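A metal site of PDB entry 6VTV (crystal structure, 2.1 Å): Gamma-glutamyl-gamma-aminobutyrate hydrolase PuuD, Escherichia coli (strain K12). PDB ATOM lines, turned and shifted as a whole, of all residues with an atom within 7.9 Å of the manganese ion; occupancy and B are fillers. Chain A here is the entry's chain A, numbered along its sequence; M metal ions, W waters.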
ATOM      1  N   LEU A 136       6.608  -0.417 -26.007  1.00  0.00           N
ATOM      2  CA  LEU A 136       7.775  -0.377 -26.888  1.00  0.00           C
ATOM      3  C   LEU A 136       8.870  -1.323 -26.393  1.00  0.00           C
ATOM      4  O   LEU A 136       9.654  -1.833 -27.192  1.00  0.00           O
ATOM      5  CB  LEU A 136       8.318   1.048 -26.993  1.00  0.00           C
ATOM      6  CG  LEU A 136       7.411   2.133 -27.578  1.00  0.00           C
ATOM      7  CD1 LEU A 136       8.088   3.490 -27.467  1.00  0.00           C
ATOM      8  CD2 LEU A 136       7.068   1.824 -29.026  1.00  0.00           C
ATOM      9  N   LEU A 143      14.995   0.658 -29.863  1.00  0.00           N
ATOM     10  CA  LEU A 143      15.860   1.147 -28.807  1.00  0.00           C
ATOM     11  C   LEU A 143      15.065   1.269 -27.497  1.00  0.00           C
ATOM     12  O   LEU A 143      13.851   1.093 -27.462  1.00  0.00           O
ATOM     13  CB  LEU A 143      16.460   2.508 -29.173  1.00  0.00           C
ATOM     14  CG  LEU A 143      17.043   2.710 -30.573  1.00  0.00           C
ATOM     15  CD1 LEU A 143      17.351   4.182 -30.798  1.00  0.00           C
ATOM     16  CD2 LEU A 143      18.280   1.867 -30.773  1.00  0.00           C
ATOM     17  N   GLU A 144      15.781   1.569 -26.424  1.00  0.00           N
ATOM     18  CA  GLU A 144      15.137   1.869 -25.148  1.00  0.00           C
ATOM     19  C   GLU A 144      14.722   3.330 -25.166  1.00  0.00           C
ATOM     20  O   GLU A 144      15.542   4.229 -25.021  1.00  0.00           O
ATOM     21  CB  GLU A 144      16.080   1.572 -23.976  1.00  0.00           C
ATOM     22  CG  GLU A 144      15.449   1.809 -22.613  1.00  0.00           C
ATOM     23  CD  GLU A 144      14.113   1.091 -22.453  1.00  0.00           C
ATOM     24  OE1 GLU A 144      13.067   1.738 -22.652  1.00  0.00           O
ATOM     25  OE2 GLU A 144      14.114  -0.111 -22.127  1.00  0.00           O
ATOM     26  N   HIS A 145      13.426   3.567 -25.367  1.00  0.00           N
ATOM     27  CA  HIS A 145      12.896   4.925 -25.444  1.00  0.00           C
ATOM     28  C   HIS A 145      12.442   5.470 -24.097  1.00  0.00           C
ATOM     29  O   HIS A 145      12.111   6.654 -24.011  1.00  0.00           O
ATOM     30  CB  HIS A 145      11.730   4.977 -26.437  1.00  0.00           C
ATOM     31  CG  HIS A 145      12.155   4.957 -27.871  1.00  0.00           C
ATOM     32  ND1 HIS A 145      12.383   6.108 -28.603  1.00  0.00           N
ATOM     33  CD2 HIS A 145      12.386   3.922 -28.712  1.00  0.00           C
ATOM     34  CE1 HIS A 145      12.742   5.775 -29.830  1.00  0.00           C
ATOM     35  NE2 HIS A 145      12.749   4.462 -29.923  1.00  0.00           N
ATOM     36  N   ARG A 146      12.426   4.640 -23.061  1.00  0.00           N
ATOM     37  CA  ARG A 146      12.013   5.074 -21.740  1.00  0.00           C
ATOM     38  C   ARG A 146      13.185   5.652 -20.975  1.00  0.00           C
ATOM     39  O   ARG A 146      14.350   5.307 -21.210  1.00  0.00           O
ATOM     40  CB  ARG A 146      11.417   3.911 -20.944  1.00  0.00           C
ATOM     41  CG  ARG A 146      10.236   3.245 -21.618  1.00  0.00           C
ATOM     42  CD  ARG A 146       9.811   1.994 -20.865  1.00  0.00           C
ATOM     43  NE  ARG A 146      10.832   0.951 -20.921  1.00  0.00           N
ATOM     44  CZ  ARG A 146      10.765  -0.190 -20.244  1.00  0.00           C
ATOM     45  NH1 ARG A 146       9.731  -0.445 -19.463  1.00  0.00           N
ATOM     46  NH2 ARG A 146      11.745  -1.085 -20.353  1.00  0.00           N
ATOM     47  N   SER A 160      19.169  11.310 -25.565  1.00  0.00           N
ATOM     48  CA  SER A 160      19.154   9.858 -25.428  1.00  0.00           C
ATOM     49  C   SER A 160      19.328   9.119 -26.753  1.00  0.00           C
ATOM     50  O   SER A 160      20.043   8.121 -26.808  1.00  0.00           O
ATOM     51  CB  SER A 160      17.843   9.403 -24.773  1.00  0.00           C
ATOM     52  OG  SER A 160      17.812   7.996 -24.622  1.00  0.00           O
ATOM     53  N   HIS A 161      18.692   9.585 -27.824  1.00  0.00           N
ATOM     54  CA  HIS A 161      18.826   8.933 -29.118  1.00  0.00           C
ATOM     55  C   HIS A 161      18.636   9.949 -30.228  1.00  0.00           C
ATOM     56  O   HIS A 161      18.171  11.076 -30.008  1.00  0.00           O
ATOM     57  CB  HIS A 161      17.843   7.758 -29.270  1.00  0.00           C
ATOM     58  CG  HIS A 161      16.400   8.166 -29.312  1.00  0.00           C
ATOM     59  ND1 HIS A 161      15.841   8.815 -30.389  1.00  0.00           N
ATOM     60  CD2 HIS A 161      15.400   8.003 -28.409  1.00  0.00           C
ATOM     61  CE1 HIS A 161      14.557   9.046 -30.154  1.00  0.00           C
ATOM     62  NE2 HIS A 161      14.265   8.566 -28.957  1.00  0.00           N
ATOM     63  N   GLU A 162      18.987   9.542 -31.436  1.00  0.00           N
ATOM     64  CA  GLU A 162      18.964  10.388 -32.614  1.00  0.00           C
ATOM     65  C   GLU A 162      17.600  10.307 -33.310  1.00  0.00           C
ATOM     66  O   GLU A 162      16.806   9.393 -33.075  1.00  0.00           O
ATOM     67  CB  GLU A 162      20.060   9.965 -33.590  1.00  0.00           C
ATOM     68  CG  GLU A 162      20.555  11.058 -34.518  1.00  0.00           C
ATOM     69  CD  GLU A 162      21.773  10.622 -35.322  1.00  0.00           C
ATOM     70  OE1 GLU A 162      22.061   9.412 -35.355  1.00  0.00           O
ATOM     71  OE2 GLU A 162      22.447  11.497 -35.916  1.00  0.00           O
ATOM     72  N   VAL A 163      17.324  11.307 -34.150  1.00  0.00           N
ATOM     73  CA  VAL A 163      16.174  11.295 -35.042  1.00  0.00           C
ATOM     74  C   VAL A 163      16.615  11.841 -36.389  1.00  0.00           C
ATOM     75  O   VAL A 163      17.522  12.668 -36.483  1.00  0.00           O
ATOM     76  CB  VAL A 163      14.984  12.107 -34.497  1.00  0.00           C
ATOM     77  CG1 VAL A 163      14.359  11.423 -33.288  1.00  0.00           C
ATOM     78  CG2 VAL A 163      15.417  13.514 -34.144  1.00  0.00           C
ATOM     79  N   VAL A 183      17.803  13.809 -29.379  1.00  0.00           N
ATOM     80  CA  VAL A 183      16.707  14.263 -28.541  1.00  0.00           C
ATOM     81  C   VAL A 183      16.628  13.376 -27.302  1.00  0.00           C
ATOM     82  O   VAL A 183      17.108  12.232 -27.292  1.00  0.00           O
ATOM     83  CB  VAL A 183      15.355  14.234 -29.287  1.00  0.00           C
ATOM     84  CG1 VAL A 183      15.346  15.260 -30.412  1.00  0.00           C
ATOM     85  CG2 VAL A 183      15.074  12.839 -29.824  1.00  0.00           C
ATOM     86  N   ASN A 184      16.022  13.912 -26.254  1.00  0.00           N
ATOM     87  CA  ASN A 184      15.704  13.106 -25.087  1.00  0.00           C
ATOM     88  C   ASN A 184      14.576  12.128 -25.416  1.00  0.00           C
ATOM     89  O   ASN A 184      13.929  12.209 -26.459  1.00  0.00           O
ATOM     90  CB  ASN A 184      15.338  13.993 -23.893  1.00  0.00           C
ATOM     91  CG  ASN A 184      14.330  15.071 -24.255  1.00  0.00           C
ATOM     92  OD1 ASN A 184      13.426  14.856 -25.070  1.00  0.00           O
ATOM     93  ND2 ASN A 184      14.485  16.247 -23.649  1.00  0.00           N
ATOM     94  N   SER A 185      14.349  11.178 -24.509  1.00  0.00           N
ATOM     95  CA  SER A 185      13.327  10.162 -24.735  1.00  0.00           C
ATOM     96  C   SER A 185      12.799   9.690 -23.390  1.00  0.00           C
ATOM     97  O   SER A 185      13.547   9.129 -22.589  1.00  0.00           O
ATOM     98  CB  SER A 185      13.903   8.989 -25.528  1.00  0.00           C
ATOM     99  OG  SER A 185      12.869   8.150 -26.017  1.00  0.00           O
ATOM    100  N   LEU A 186      11.507   9.918 -23.153  1.00  0.00           N
ATOM    101  CA  LEU A 186      10.869   9.563 -21.881  1.00  0.00           C
ATOM    102  C   LEU A 186       9.481   8.980 -22.144  1.00  0.00           C
ATOM    103  O   LEU A 186       8.475   9.450 -21.612  1.00  0.00           O
ATOM    104  CB  LEU A 186      10.789  10.769 -20.942  1.00  0.00           C
ATOM    105  CG  LEU A 186      12.061  11.533 -20.563  1.00  0.00           C
ATOM    106  CD1 LEU A 186      12.383  12.628 -21.571  1.00  0.00           C
ATOM    107  CD2 LEU A 186      11.926  12.113 -19.164  1.00  0.00           C
ATOM    108  N   HIS A 187       9.406   7.941 -22.973  1.00  0.00           N
ATOM    109  CA  HIS A 187       8.125   7.374 -23.365  1.00  0.00           C
ATOM    110  C   HIS A 187       8.222   5.873 -23.509  1.00  0.00           C
ATOM    111  O   HIS A 187       9.212   5.359 -24.046  1.00  0.00           O
ATOM    112  CB  HIS A 187       7.624   7.999 -24.671  1.00  0.00           C
ATOM    113  CG  HIS A 187       8.548   7.809 -25.828  1.00  0.00           C
ATOM    114  ND1 HIS A 187       8.270   6.952 -26.877  1.00  0.00           N
ATOM    115  CD2 HIS A 187       9.758   8.362 -26.113  1.00  0.00           C
ATOM    116  CE1 HIS A 187       9.262   6.992 -27.750  1.00  0.00           C
ATOM    117  NE2 HIS A 187      10.173   7.831 -27.310  1.00  0.00           N
ATOM    118  N   GLY A 188       7.195   5.167 -23.039  1.00  0.00           N
ATOM    119  CA  GLY A 188       7.140   3.726 -23.155  1.00  0.00           C
ATOM    120  C   GLY A 188       6.166   3.305 -24.222  1.00  0.00           C
ATOM    121  O   GLY A 188       6.035   2.115 -24.550  1.00  0.00           O
ATOM    122  N   GLN A 189       5.461   4.287 -24.786  1.00  0.00           N
ATOM    123  CA  GLN A 189       4.533   4.087 -25.879  1.00  0.00           C
ATOM    124  C   GLN A 189       4.964   4.930 -27.064  1.00  0.00           C
ATOM    125  O   GLN A 189       5.660   5.937 -26.924  1.00  0.00           O
ATOM    126  CB  GLN A 189       3.085   4.439 -25.462  1.00  0.00           C
ATOM    127  CG  GLN A 189       2.530   3.567 -24.342  1.00  0.00           C
ATOM    128  CD  GLN A 189       1.017   3.652 -24.219  1.00  0.00           C
ATOM    129  OE1 GLN A 189       0.387   4.504 -24.840  1.00  0.00           O
ATOM    130  NE2 GLN A 189       0.440   2.763 -23.417  1.00  0.00           N
ATOM    131  N   SER A 204      13.438   7.795 -35.346  1.00  0.00           N
ATOM    132  CA  SER A 204      14.655   7.359 -34.686  1.00  0.00           C
ATOM    133  C   SER A 204      15.299   6.248 -35.506  1.00  0.00           C
ATOM    134  O   SER A 204      14.680   5.680 -36.404  1.00  0.00           O
ATOM    135  CB  SER A 204      14.323   6.911 -33.264  1.00  0.00           C
ATOM    136  OG  SER A 204      13.105   6.190 -33.229  1.00  0.00           O
ATOM    137  N   ASP A 206      15.771   3.208 -35.071  1.00  0.00           N
ATOM    138  CA  ASP A 206      15.043   1.958 -35.067  1.00  0.00           C
ATOM    139  C   ASP A 206      13.783   1.990 -35.927  1.00  0.00           C
ATOM    140  O   ASP A 206      13.087   0.983 -36.017  1.00  0.00           O
ATOM    141  CB  ASP A 206      14.686   1.552 -33.628  1.00  0.00           C
ATOM    142  CG  ASP A 206      13.976   2.656 -32.872  1.00  0.00           C
ATOM    143  OD1 ASP A 206      13.598   3.673 -33.494  1.00  0.00           O
ATOM    144  OD2 ASP A 206      13.803   2.516 -31.645  1.00  0.00           O
ATOM    145  N   LEU A 208      11.104   4.006 -35.430  1.00  0.00           N
ATOM    146  CA  LEU A 208       9.924   4.505 -34.735  1.00  0.00           C
ATOM    147  C   LEU A 208       9.673   5.970 -35.095  1.00  0.00           C
ATOM    148  O   LEU A 208      10.598   6.787 -35.129  1.00  0.00           O
ATOM    149  CB  LEU A 208      10.094   4.363 -33.223  1.00  0.00           C
ATOM    150  CG  LEU A 208       8.866   4.754 -32.398  1.00  0.00           C
ATOM    151  CD1 LEU A 208       7.843   3.629 -32.391  1.00  0.00           C
ATOM    152  CD2 LEU A 208       9.273   5.132 -30.984  1.00  0.00           C
ATOM    153  N   VAL A 209       8.412   6.295 -35.372  1.00  0.00           N
ATOM    154  CA  VAL A 209       8.044   7.658 -35.702  1.00  0.00           C
ATOM    155  C   VAL A 209       8.192   8.533 -34.464  1.00  0.00           C
ATOM    156  O   VAL A 209       7.622   8.247 -33.402  1.00  0.00           O
ATOM    157  CB  VAL A 209       6.621   7.721 -36.248  1.00  0.00           C
ATOM    158  CG1 VAL A 209       6.138   9.157 -36.317  1.00  0.00           C
ATOM    159  CG2 VAL A 209       6.550   7.066 -37.621  1.00  0.00           C
ATOM    160  N   GLU A 210       8.973   9.616 -34.589  1.00  0.00           N
ATOM    161  CA  GLU A 210       9.210  10.524 -33.481  1.00  0.00           C
ATOM    162  C   GLU A 210       8.636  11.912 -33.699  1.00  0.00           C
ATOM    163  O   GLU A 210       8.733  12.755 -32.794  1.00  0.00           O
ATOM    164  CB  GLU A 210      10.715  10.634 -33.186  1.00  0.00           C
ATOM    165  CG  GLU A 210      11.287   9.397 -32.504  1.00  0.00           C
ATOM    166  CD  GLU A 210      11.297   9.531 -30.990  1.00  0.00           C
ATOM    167  OE1 GLU A 210      11.214  10.670 -30.480  1.00  0.00           O
ATOM    168  OE2 GLU A 210      11.380   8.484 -30.309  1.00  0.00           O
ATOM    169  N   GLN A 224       7.714  13.451 -30.341  1.00  0.00           N
ATOM    170  CA  GLN A 224       7.707  12.417 -29.300  1.00  0.00           C
ATOM    171  C   GLN A 224       8.640  12.747 -28.140  1.00  0.00           C
ATOM    172  O   GLN A 224       8.418  12.239 -27.029  1.00  0.00           O
ATOM    173  CB  GLN A 224       8.085  11.071 -29.915  1.00  0.00           C
ATOM    174  CG  GLN A 224       7.978   9.872 -28.983  1.00  0.00           C
ATOM    175  CD  GLN A 224       6.588   9.651 -28.438  1.00  0.00           C
ATOM    176  OE1 GLN A 224       5.762   8.965 -29.050  1.00  0.00           O
ATOM    177  NE2 GLN A 224       6.300  10.228 -27.278  1.00  0.00           N
ATOM    178  N   TRP A 225       9.645  13.592 -28.353  1.00  0.00           N
ATOM    179  CA  TRP A 225      10.580  13.946 -27.287  1.00  0.00           C
ATOM    180  C   TRP A 225      10.030  15.136 -26.493  1.00  0.00           C
ATOM    181  O   TRP A 225       8.875  15.535 -26.653  1.00  0.00           O
ATOM    182  CB  TRP A 225      11.958  14.224 -27.877  1.00  0.00           C
ATOM    183  CG  TRP A 225      12.035  15.382 -28.818  1.00  0.00           C
ATOM    184  CD1 TRP A 225      12.340  16.679 -28.506  1.00  0.00           C
ATOM    185  CD2 TRP A 225      11.804  15.354 -30.231  1.00  0.00           C
ATOM    186  NE1 TRP A 225      12.324  17.452 -29.640  1.00  0.00           N
ATOM    187  CE2 TRP A 225      11.988  16.668 -30.713  1.00  0.00           C
ATOM    188  CE3 TRP A 225      11.456  14.347 -31.134  1.00  0.00           C
ATOM    189  CZ2 TRP A 225      11.846  16.992 -32.059  1.00  0.00           C
ATOM    190  CZ3 TRP A 225      11.314  14.677 -32.472  1.00  0.00           C
ATOM    191  CH2 TRP A 225      11.508  15.982 -32.921  1.00  0.00           C
HETATM  192 MN    MN M   1      12.185   8.255 -28.205  1.00  0.00          MN
HETATM  193  O   HOH W   1      12.022  10.567 -27.841  1.00  0.00           O
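N of Arg 146 lies close to O of His 187.
A ring nitrogen (NE2) of His 145 sits at hydrogen-bond distance from the side-chain carboxylate (OD2) of Asp 206, 2.8 Å away.
The backbone carbonyl oxygen of His 161 lies within hydrogen-bond range of the backbone NH of Val 183, at 2.8 Å.
N of Leu 186 is in hydrogen-bond range of O of His 145 (3.4 Å).
A ring nitrogen (ND1) of His 187 lies within hydrogen-bond range of the backbone carbonyl oxygen of Gln 189.
The backbone carbonyl oxygen (O) of Glu 210 sits at hydrogen-bond distance from the backbone NH (N) of Gln 224, 2.7 Å away.
The nearest printed residue that does not touch the manganese ion is Gln 224 (4.6 Å).
The manganese ion is bound by a ring nitrogen (ND1) of His 145, a ring nitrogen (NE2) of His 161, a ring nitrogen (NE2) of His 187, the side-chain carboxylate of Glu 210, the side-chain hydroxyl of Ser 185 and water W1.
Water W1 lies within hydrogen-bond range of OE1 of Glu 210 (2.8 Å) and O of Asn 184 (2.9 Å).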
